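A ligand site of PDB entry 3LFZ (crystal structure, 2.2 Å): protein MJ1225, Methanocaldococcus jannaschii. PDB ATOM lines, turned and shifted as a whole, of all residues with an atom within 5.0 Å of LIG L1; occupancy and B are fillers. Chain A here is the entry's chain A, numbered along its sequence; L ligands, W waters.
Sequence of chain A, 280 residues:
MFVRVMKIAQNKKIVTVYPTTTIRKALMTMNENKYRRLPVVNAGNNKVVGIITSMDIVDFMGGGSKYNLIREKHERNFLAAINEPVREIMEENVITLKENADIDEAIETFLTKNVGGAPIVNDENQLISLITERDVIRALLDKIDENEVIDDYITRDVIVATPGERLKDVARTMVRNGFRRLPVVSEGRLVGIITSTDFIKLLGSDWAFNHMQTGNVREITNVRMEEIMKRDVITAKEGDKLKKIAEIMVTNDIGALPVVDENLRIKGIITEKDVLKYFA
The side-chain hydroxyl of Thr 53 lies within hydrogen-bond range of an oxygen (O7) of LIG L1 (2.9 Å).
N3 of LG2 L2 lies within hydrogen-bond range of O of Arg 181 (3.2 Å).
The guanidinium group of Arg 37 is in salt-bridge range of an oxygen (O5) of LIG L1.
O of Ile 95 sits at hydrogen-bond distance from N3 of LIG L1 (3.1 Å).
N3 of LIG L1 sits at hydrogen-bond distance from O of Gly 117, at 3.1 Å.
N of Gly 116 lies within hydrogen-bond range of O5 of LIG L1, 2.5 Å away.
The backbone NH (N) of Ile 95 is in hydrogen-bond range of a nitrogen (N4) of LIG L1, 2.8 Å away.
An oxygen (O1) of LG2 L2 lies within salt-bridge range of the guanidinium group of Arg 181 (2.7 Å).
The backbone NH of Arg 181 sits at hydrogen-bond distance from an oxygen (O2) of LG2 L2, at 3.2 Å.
The side-chain carboxylate (OD1) of Asp 56 is in hydrogen-bond range of an oxygen (O12) of LIG L1 (2.4 Å).
The guanidinium group (NH2) of Arg 181 is in salt-bridge range of an oxygen (O3) of LIG L1, at 3.7 Å.
The guanidinium group (NH1) of Arg 180 is in salt-bridge range of an oxygen (O3) of LIG L1 (3.5 Å).
N of Arg 180 sits at hydrogen-bond distance from O3 of LG2 L2 (3.0 Å).
O1 of LIG L1 sits close to O3 of LG2 L2, at 2.6 Å.
The backbone carbonyl oxygen (O) of Val 115 is in hydrogen-bond range of the side-chain amino group (NZ) of Lys 273 (2.9 Å).
The side-chain carboxylate (OE1) of Glu 133 lies within salt-bridge range of the side-chain amino group (NZ) of Lys 273 (2.8 Å).
The side-chain hydroxyl of Thr 53 sits close to the backbone NH of Met 55, 3.1 Å away.
NZ of Lys 66 lies within salt-bridge range of OD1 of Asp 56 (2.9 Å).
The backbone carbonyl oxygen (O) of Gly 117 sits at hydrogen-bond distance from the guanidinium group (NH1) of Arg 37 (3.4 Å).
The side-chain amino group (NZ) of Lys 66 lies within salt-bridge range of the side-chain carboxylate (OE2) of Glu 91.
The backbone NH (N) of Thr 53 lies within hydrogen-bond range of the side-chain carboxylate (OD2) of Asp 56 (2.9 Å).
N of Glu 91 sits at hydrogen-bond distance from O of Ile 51 (2.9 Å).
OE2 of Glu 133 lies close to O2 of LIG L1 (3.5 Å).
Ile 51 touches LIG L1 (CG2 to C10, 3.7 Å).
Met 55 touches LIG L1 (CB to O10, 3.3 Å).
Glu 91 touches LIG L1 (CG to O13, 3.1 Å).
CG1 of Val 94 touches N4 of LIG L1, at 3.4 Å.
Asn 114 touches LIG L1.
Val 115 touches LIG L1.
Pro 119 touches LIG L1.
Water W2 lies within hydrogen-bond range of the side-chain carboxylate (OE2) of Glu 133 (2.4 Å), an oxygen (O4) of LG2 L2 (2.4 Å), an oxygen (O2) of LIG L1 (2.6 Å) and the side-chain amino group (NZ) of Lys 273 (3.5 Å).
Water W1 lies within hydrogen-bond range of an oxygen (O2) of LIG L1, the side-chain amino group of Lys 273, an oxygen (O5) of LG2 L2 and the backbone carbonyl oxygen of Asn 114.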
ATOM      1  N   ARG A  37     -14.757  -0.282  -9.273  1.00  0.00           N
ATOM      2  CA  ARG A  37     -15.531  -0.801  -8.125  1.00  0.00           C
ATOM      3  C   ARG A  37     -15.193  -2.268  -7.830  1.00  0.00           C
ATOM      4  O   ARG A  37     -15.469  -3.150  -8.649  1.00  0.00           O
ATOM      5  CB  ARG A  37     -17.028  -0.631  -8.380  1.00  0.00           C
ATOM      6  CG  ARG A  37     -17.927  -1.029  -7.209  1.00  0.00           C
ATOM      7  CD  ARG A  37     -19.384  -1.182  -7.653  1.00  0.00           C
ATOM      8  NE  ARG A  37     -19.828  -0.053  -8.467  1.00  0.00           N
ATOM      9  CZ  ARG A  37     -20.446   1.032  -8.002  1.00  0.00           C
ATOM     10  NH1 ARG A  37     -20.713   1.147  -6.706  1.00  0.00           N
ATOM     11  NH2 ARG A  37     -20.803   1.992  -8.832  1.00  0.00           N
ATOM     12  N   ILE A  51     -16.545  -3.497   0.135  1.00  0.00           N
ATOM     13  CA  ILE A  51     -16.459  -2.959  -1.217  1.00  0.00           C
ATOM     14  C   ILE A  51     -15.521  -1.750  -1.182  1.00  0.00           C
ATOM     15  O   ILE A  51     -15.483  -1.011  -0.196  1.00  0.00           O
ATOM     16  CB  ILE A  51     -17.867  -2.605  -1.807  1.00  0.00           C
ATOM     17  CG1 ILE A  51     -17.793  -2.302  -3.306  1.00  0.00           C
ATOM     18  CG2 ILE A  51     -18.545  -1.460  -1.018  1.00  0.00           C
ATOM     19  CD1 ILE A  51     -19.092  -2.569  -4.061  1.00  0.00           C
ATOM     20  N   ILE A  52     -14.743  -1.583  -2.240  1.00  0.00           N
ATOM     21  CA  ILE A  52     -13.859  -0.435  -2.351  1.00  0.00           C
ATOM     22  C   ILE A  52     -13.939   0.159  -3.754  1.00  0.00           C
ATOM     23  O   ILE A  52     -13.818  -0.562  -4.761  1.00  0.00           O
ATOM     24  CB  ILE A  52     -12.395  -0.768  -1.946  1.00  0.00           C
ATOM     25  CG1 ILE A  52     -11.533   0.493  -1.992  1.00  0.00           C
ATOM     26  CG2 ILE A  52     -11.804  -1.891  -2.817  1.00  0.00           C
ATOM     27  CD1 ILE A  52     -10.460   0.523  -0.957  1.00  0.00           C
ATOM     28  N   THR A  53     -14.191   1.467  -3.824  1.00  0.00           N
ATOM     29  CA  THR A  53     -14.293   2.170  -5.091  1.00  0.00           C
ATOM     30  C   THR A  53     -13.219   3.242  -5.157  1.00  0.00           C
ATOM     31  O   THR A  53     -12.485   3.478  -4.198  1.00  0.00           O
ATOM     32  CB  THR A  53     -15.677   2.833  -5.293  1.00  0.00           C
ATOM     33  OG1 THR A  53     -15.817   3.974  -4.438  1.00  0.00           O
ATOM     34  CG2 THR A  53     -16.815   1.847  -5.024  1.00  0.00           C
ATOM     35  N   SER A  54     -13.150   3.906  -6.312  1.00  0.00           N
ATOM     36  CA  SER A  54     -12.230   5.019  -6.509  1.00  0.00           C
ATOM     37  C   SER A  54     -12.526   6.160  -5.542  1.00  0.00           C
ATOM     38  O   SER A  54     -11.621   6.914  -5.179  1.00  0.00           O
ATOM     39  CB  SER A  54     -12.272   5.524  -7.956  1.00  0.00           C
ATOM     40  OG  SER A  54     -13.531   6.084  -8.261  1.00  0.00           O
ATOM     41  N   MET A  55     -13.786   6.276  -5.132  1.00  0.00           N
ATOM     42  CA  MET A  55     -14.176   7.285  -4.144  1.00  0.00           C
ATOM     43  C   MET A  55     -13.541   7.046  -2.773  1.00  0.00           C
ATOM     44  O   MET A  55     -13.171   8.005  -2.095  1.00  0.00           O
ATOM     45  CB  MET A  55     -15.695   7.395  -4.027  1.00  0.00           C
ATOM     46  CG  MET A  55     -16.317   8.464  -4.912  1.00  0.00           C
ATOM     47  SD  MET A  55     -15.956  10.151  -4.372  1.00  0.00           S
ATOM     48  CE  MET A  55     -14.640  10.601  -5.483  1.00  0.00           C
ATOM     49  N   ASP A  56     -13.403   5.780  -2.385  1.00  0.00           N
ATOM     50  CA  ASP A  56     -12.689   5.440  -1.143  1.00  0.00           C
ATOM     51  C   ASP A  56     -11.208   5.789  -1.235  1.00  0.00           C
ATOM     52  O   ASP A  56     -10.590   6.176  -0.243  1.00  0.00           O
ATOM     53  CB  ASP A  56     -12.863   3.963  -0.819  1.00  0.00           C
ATOM     54  CG  ASP A  56     -14.300   3.582  -0.580  1.00  0.00           C
ATOM     55  OD1 ASP A  56     -14.945   4.214   0.285  1.00  0.00           O
ATOM     56  OD2 ASP A  56     -14.787   2.651  -1.263  1.00  0.00           O
ATOM     57  N   LYS A  66     -10.569   9.016   5.842  1.00  0.00           N
ATOM     58  CA  LYS A  66      -9.624   7.915   5.597  1.00  0.00           C
ATOM     59  C   LYS A  66      -8.180   8.391   5.387  1.00  0.00           C
ATOM     60  O   LYS A  66      -7.236   7.617   5.538  1.00  0.00           O
ATOM     61  CB  LYS A  66     -10.119   7.023   4.449  1.00  0.00           C
ATOM     62  CG  LYS A  66     -11.380   6.254   4.809  1.00  0.00           C
ATOM     63  CD  LYS A  66     -12.073   5.622   3.611  1.00  0.00           C
ATOM     64  CE  LYS A  66     -13.498   5.233   4.003  1.00  0.00           C
ATOM     65  NZ  LYS A  66     -14.108   4.251   3.075  1.00  0.00           N
ATOM     66  N   GLU A  91     -15.486  -0.008   2.511  1.00  0.00           N
ATOM     67  CA  GLU A  91     -16.807   0.143   3.094  1.00  0.00           C
ATOM     68  C   GLU A  91     -17.359  -1.219   3.472  1.00  0.00           C
ATOM     69  O   GLU A  91     -17.288  -2.159   2.685  1.00  0.00           O
ATOM     70  CB  GLU A  91     -17.749   0.858   2.129  1.00  0.00           C
ATOM     71  CG  GLU A  91     -17.481   2.347   2.017  1.00  0.00           C
ATOM     72  CD  GLU A  91     -17.787   3.091   3.303  1.00  0.00           C
ATOM     73  OE1 GLU A  91     -18.978   3.115   3.704  1.00  0.00           O
ATOM     74  OE2 GLU A  91     -16.852   3.652   3.917  1.00  0.00           O
ATOM     75  N   ASN A  93     -20.832  -3.274   5.629  1.00  0.00           N
ATOM     76  CA  ASN A  93     -22.292  -3.149   5.592  1.00  0.00           C
ATOM     77  C   ASN A  93     -22.724  -2.811   4.152  1.00  0.00           C
ATOM     78  O   ASN A  93     -23.403  -1.817   3.897  1.00  0.00           O
ATOM     79  CB  ASN A  93     -22.756  -2.070   6.590  1.00  0.00           C
ATOM     80  CG  ASN A  93     -24.275  -2.070   6.820  1.00  0.00           C
ATOM     81  OD1 ASN A  93     -24.957  -3.057   6.569  1.00  0.00           O
ATOM     82  ND2 ASN A  93     -24.786  -0.943   7.308  1.00  0.00           N
ATOM     83  N   VAL A  94     -22.287  -3.656   3.206  1.00  0.00           N
ATOM     84  CA  VAL A  94     -22.463  -3.416   1.769  1.00  0.00           C
ATOM     85  C   VAL A  94     -23.929  -3.498   1.333  1.00  0.00           C
ATOM     86  O   VAL A  94     -24.684  -4.330   1.845  1.00  0.00           O
ATOM     87  CB  VAL A  94     -21.624  -4.430   0.935  1.00  0.00           C
ATOM     88  CG1 VAL A  94     -21.718  -4.147  -0.573  1.00  0.00           C
ATOM     89  CG2 VAL A  94     -20.179  -4.422   1.381  1.00  0.00           C
ATOM     90  N   ILE A  95     -24.332  -2.646   0.399  1.00  0.00           N
ATOM     91  CA  ILE A  95     -25.658  -2.775  -0.211  1.00  0.00           C
ATOM     92  C   ILE A  95     -25.607  -3.787  -1.361  1.00  0.00           C
ATOM     93  O   ILE A  95     -24.956  -3.549  -2.386  1.00  0.00           O
ATOM     94  CB  ILE A  95     -26.211  -1.419  -0.701  1.00  0.00           C
ATOM     95  CG1 ILE A  95     -26.333  -0.443   0.481  1.00  0.00           C
ATOM     96  CG2 ILE A  95     -27.581  -1.598  -1.365  1.00  0.00           C
ATOM     97  CD1 ILE A  95     -26.562   0.998   0.079  1.00  0.00           C
ATOM     98  N   ASN A 114     -28.385   5.815  -3.160  1.00  0.00           N
ATOM     99  CA  ASN A 114     -27.190   6.494  -3.656  1.00  0.00           C
ATOM    100  C   ASN A 114     -26.011   5.554  -3.926  1.00  0.00           C
ATOM    101  O   ASN A 114     -24.889   5.803  -3.475  1.00  0.00           O
ATOM    102  CB  ASN A 114     -26.796   7.630  -2.697  1.00  0.00           C
ATOM    103  CG  ASN A 114     -25.850   8.638  -3.311  1.00  0.00           C
ATOM    104  OD1 ASN A 114     -25.856   8.857  -4.526  1.00  0.00           O
ATOM    105  ND2 ASN A 114     -25.028   9.271  -2.481  1.00  0.00           N
ATOM    106  N   VAL A 115     -26.274   4.450  -4.628  1.00  0.00           N
ATOM    107  CA  VAL A 115     -25.217   3.587  -5.157  1.00  0.00           C
ATOM    108  C   VAL A 115     -25.393   3.439  -6.676  1.00  0.00           C
ATOM    109  O   VAL A 115     -26.498   3.589  -7.195  1.00  0.00           O
ATOM    110  CB  VAL A 115     -25.165   2.178  -4.494  1.00  0.00           C
ATOM    111  CG1 VAL A 115     -24.792   2.290  -3.021  1.00  0.00           C
ATOM    112  CG2 VAL A 115     -26.486   1.417  -4.666  1.00  0.00           C
ATOM    113  N   GLY A 116     -24.299   3.143  -7.374  1.00  0.00           N
ATOM    114  CA  GLY A 116     -24.331   2.980  -8.825  1.00  0.00           C
ATOM    115  C   GLY A 116     -24.104   1.551  -9.269  1.00  0.00           C
ATOM    116  O   GLY A 116     -24.186   1.255 -10.461  1.00  0.00           O
ATOM    117  N   GLY A 117     -23.808   0.680  -8.317  1.00  0.00           N
ATOM    118  CA  GLY A 117     -23.516  -0.721  -8.614  1.00  0.00           C
ATOM    119  C   GLY A 117     -23.653  -1.531  -7.342  1.00  0.00           C
ATOM    120  O   GLY A 117     -23.284  -1.057  -6.271  1.00  0.00           O
ATOM    121  N   ALA A 118     -24.188  -2.732  -7.460  1.00  0.00           N
ATOM    122  CA  ALA A 118     -24.373  -3.573  -6.285  1.00  0.00           C
ATOM    123  C   ALA A 118     -24.006  -5.035  -6.551  1.00  0.00           C
ATOM    124  O   ALA A 118     -24.353  -5.578  -7.608  1.00  0.00           O
ATOM    125  CB  ALA A 118     -25.801  -3.473  -5.774  1.00  0.00           C
ATOM    126  N   PRO A 119     -23.302  -5.665  -5.596  1.00  0.00           N
ATOM    127  CA  PRO A 119     -23.020  -7.088  -5.661  1.00  0.00           C
ATOM    128  C   PRO A 119     -24.307  -7.893  -5.586  1.00  0.00           C
ATOM    129  O   PRO A 119     -25.228  -7.546  -4.828  1.00  0.00           O
ATOM    130  CB  PRO A 119     -22.168  -7.334  -4.414  1.00  0.00           C
ATOM    131  CG  PRO A 119     -21.588  -6.006  -4.082  1.00  0.00           C
ATOM    132  CD  PRO A 119     -22.655  -5.033  -4.434  1.00  0.00           C
ATOM    133  N   GLU A 133     -25.760   0.615 -12.762  1.00  0.00           N
ATOM    134  CA  GLU A 133     -26.748   1.435 -13.443  1.00  0.00           C
ATOM    135  C   GLU A 133     -26.576   1.372 -14.962  1.00  0.00           C
ATOM    136  O   GLU A 133     -27.547   1.458 -15.705  1.00  0.00           O
ATOM    137  CB  GLU A 133     -26.651   2.889 -12.980  1.00  0.00           C
ATOM    138  CG  GLU A 133     -26.863   3.075 -11.489  1.00  0.00           C
ATOM    139  CD  GLU A 133     -26.616   4.503 -11.048  1.00  0.00           C
ATOM    140  OE1 GLU A 133     -27.520   5.088 -10.434  1.00  0.00           O
ATOM    141  OE2 GLU A 133     -25.509   5.030 -11.309  1.00  0.00           O
ATOM    142  N   GLY A 178     -20.402  13.463  -2.331  1.00  0.00           N
ATOM    143  CA  GLY A 178     -20.646  12.131  -2.895  1.00  0.00           C
ATOM    144  C   GLY A 178     -20.740  12.136  -4.417  1.00  0.00           C
ATOM    145  O   GLY A 178     -21.447  11.319  -4.998  1.00  0.00           O
ATOM    146  N   ARG A 180     -18.588  11.771  -7.888  1.00  0.00           N
ATOM    147  CA  ARG A 180     -17.336  11.320  -8.493  1.00  0.00           C
ATOM    148  C   ARG A 180     -16.851  12.241  -9.614  1.00  0.00           C
ATOM    149  O   ARG A 180     -15.652  12.315  -9.885  1.00  0.00           O
ATOM    150  CB  ARG A 180     -17.478   9.907  -9.053  1.00  0.00           C
ATOM    151  CG  ARG A 180     -18.035   8.887  -8.069  1.00  0.00           C
ATOM    152  CD  ARG A 180     -17.910   7.484  -8.647  1.00  0.00           C
ATOM    153  NE  ARG A 180     -16.737   7.378  -9.491  1.00  0.00           N
ATOM    154  CZ  ARG A 180     -16.768   7.063 -10.788  1.00  0.00           C
ATOM    155  NH1 ARG A 180     -17.927   6.777 -11.374  1.00  0.00           N
ATOM    156  NH2 ARG A 180     -15.640   7.007 -11.477  1.00  0.00           N
ATOM    157  N   ARG A 181     -17.773  12.920 -10.284  1.00  0.00           N
ATOM    158  CA  ARG A 181     -17.379  13.832 -11.355  1.00  0.00           C
ATOM    159  C   ARG A 181     -17.834  15.253 -11.160  1.00  0.00           C
ATOM    160  O   ARG A 181     -18.989  15.521 -10.821  1.00  0.00           O
ATOM    161  CB  ARG A 181     -17.772  13.349 -12.752  1.00  0.00           C
ATOM    162  CG  ARG A 181     -18.997  12.505 -12.800  1.00  0.00           C
ATOM    163  CD  ARG A 181     -18.595  11.062 -12.830  1.00  0.00           C
ATOM    164  NE  ARG A 181     -19.772  10.231 -12.872  1.00  0.00           N
ATOM    165  CZ  ARG A 181     -19.737   8.923 -13.090  1.00  0.00           C
ATOM    166  NH1 ARG A 181     -18.568   8.328 -13.269  1.00  0.00           N
ATOM    167  NH2 ARG A 181     -20.859   8.212 -13.119  1.00  0.00           N
ATOM    168  N   LYS A 273     -27.737   7.878 -13.142  1.00  0.00           N
ATOM    169  CA  LYS A 273     -28.797   7.782 -12.139  1.00  0.00           C
ATOM    170  C   LYS A 273     -30.028   8.583 -12.567  1.00  0.00           C
ATOM    171  O   LYS A 273     -31.150   8.137 -12.379  1.00  0.00           O
ATOM    172  CB  LYS A 273     -28.318   8.238 -10.762  1.00  0.00           C
ATOM    173  CG  LYS A 273     -29.218   7.753  -9.620  1.00  0.00           C
ATOM    174  CD  LYS A 273     -28.781   8.254  -8.249  1.00  0.00           C
ATOM    175  CE  LYS A 273     -27.407   7.725  -7.850  1.00  0.00           C
ATOM    176  NZ  LYS A 273     -27.305   6.239  -7.905  1.00  0.00           N
HETATM  177  P1  LIG L   1     -21.687   6.150  -8.991  1.00  0.00           P
HETATM  178  O1  LIG L   1     -21.193   7.669  -8.794  1.00  0.00           O
HETATM  179  O2  LIG L   1     -23.157   6.035  -8.933  1.00  0.00           O
HETATM  180  O3  LIG L   1     -21.108   5.737 -10.443  1.00  0.00           O
HETATM  181  P2  LIG L   1     -21.386   4.891  -6.398  1.00  0.00           P
HETATM  182  O4  LIG L   1     -22.081   6.036  -5.762  1.00  0.00           O
HETATM  183  O5  LIG L   1     -22.045   3.579  -6.448  1.00  0.00           O
HETATM  184  O6  LIG L   1     -20.858   5.284  -7.885  1.00  0.00           O
HETATM  185  P3  LIG L   1     -18.855   5.735  -5.498  1.00  0.00           P
HETATM  186  O7  LIG L   1     -17.694   5.266  -6.285  1.00  0.00           O
HETATM  187  O8  LIG L   1     -19.391   7.096  -5.714  1.00  0.00           O
HETATM  188  O9  LIG L   1     -20.003   4.633  -5.631  1.00  0.00           O
HETATM  189  O10 LIG L   1     -18.450   5.562  -3.944  1.00  0.00           O
HETATM  190  C1  LIG L   1     -19.055   6.314  -2.875  1.00  0.00           C
HETATM  191  C2  LIG L   1     -19.033   5.480  -1.585  1.00  0.00           C
HETATM  192  O11 LIG L   1     -20.078   4.476  -1.718  1.00  0.00           O
HETATM  193  C3  LIG L   1     -17.706   4.724  -1.408  1.00  0.00           C
HETATM  194  O12 LIG L   1     -17.297   4.815  -0.041  1.00  0.00           O
HETATM  195  C4  LIG L   1     -18.059   3.286  -1.791  1.00  0.00           C
HETATM  196  O13 LIG L   1     -17.251   2.338  -1.088  1.00  0.00           O
HETATM  197  C5  LIG L   1     -19.522   3.201  -1.340  1.00  0.00           C
HETATM  198  N1  LIG L   1     -20.268   2.160  -2.082  1.00  0.00           N
HETATM  199  C6  LIG L   1     -20.328   1.997  -3.415  1.00  0.00           C
HETATM  200  N2  LIG L   1     -21.099   0.955  -3.706  1.00  0.00           N
HETATM  201  C7  LIG L   1     -21.552   0.452  -2.560  1.00  0.00           C
HETATM  202  C8  LIG L   1     -22.386  -0.611  -2.234  1.00  0.00           C
HETATM  203  N3  LIG L   1     -22.926  -1.393  -3.168  1.00  0.00           N
HETATM  204  N4  LIG L   1     -22.653  -0.851  -0.931  1.00  0.00           N
HETATM  205  C9  LIG L   1     -22.125  -0.098   0.022  1.00  0.00           C
HETATM  206  N5  LIG L   1     -21.321   0.920  -0.256  1.00  0.00           N
HETATM  207  C10 LIG L   1     -21.027   1.214  -1.537  1.00  0.00           C
HETATM  208  P1  LG2 L   2     -21.732  10.995  -9.810  1.00  0.00           P
HETATM  209  O1  LG2 L   2     -21.710  10.190 -11.049  1.00  0.00           O
HETATM  210  O2  LG2 L   2     -20.915  12.389  -9.975  1.00  0.00           O
HETATM  211  O3  LG2 L   2     -21.110  10.276  -8.490  1.00  0.00           O
HETATM  212  P2  LG2 L   2     -24.389  10.260  -9.438  1.00  0.00           P
HETATM  213  O4  LG2 L   2     -24.502   9.565 -10.746  1.00  0.00           O
HETATM  214  O5  LG2 L   2     -24.095   9.280  -8.172  1.00  0.00           O
HETATM  215  O6  LG2 L   2     -23.216  11.376  -9.413  1.00  0.00           O
HETATM  216  O7  LG2 L   2     -25.697  11.153  -9.253  1.00  0.00           O
HETATM  217  C1  LG2 L   2     -26.475  11.347  -8.081  1.00  0.00           C
HETATM  218  C2  LG2 L   2     -27.251  12.666  -8.275  1.00  0.00           C
HETATM  219  O8  LG2 L   2     -26.301  13.749  -8.034  1.00  0.00           O
HETATM  220  C3  LG2 L   2     -27.771  12.844  -9.711  1.00  0.00           C
HETATM  221  O9  LG2 L   2     -29.046  13.507  -9.688  1.00  0.00           O
HETATM  222  C4  LG2 L   2     -26.721  13.735 -10.361  1.00  0.00           C
HETATM  223  O10 LG2 L   2     -27.274  14.521 -11.422  1.00  0.00           O
HETATM  224  C5  LG2 L   2     -26.271  14.621  -9.198  1.00  0.00           C
HETATM  225  N1  LG2 L   2     -24.882  15.118  -9.445  1.00  0.00           N
HETATM  226  C6  LG2 L   2     -23.856  14.416  -9.941  1.00  0.00           C
HETATM  227  N2  LG2 L   2     -22.772  15.189 -10.019  1.00  0.00           N
HETATM  228  C7  LG2 L   2     -23.108  16.398  -9.583  1.00  0.00           C
HETATM  229  C8  LG2 L   2     -22.417  17.590  -9.436  1.00  0.00           C
HETATM  230  N3  LG2 L   2     -21.136  17.693  -9.768  1.00  0.00           N
HETATM  231  N4  LG2 L   2     -23.080  18.655  -8.935  1.00  0.00           N
HETATM  232  C9  LG2 L   2     -24.358  18.574  -8.593  1.00  0.00           C
HETATM  233  N5  LG2 L   2     -25.042  17.441  -8.731  1.00  0.00           N
HETATM  234  C10 LG2 L   2     -24.442  16.347  -9.218  1.00  0.00           C
HETATM  235  O   HOH W   1     -24.541   6.606  -6.785  1.00  0.00           O
HETATM  236  O   HOH W   2     -25.002   7.206 -10.320  1.00  0.00           O
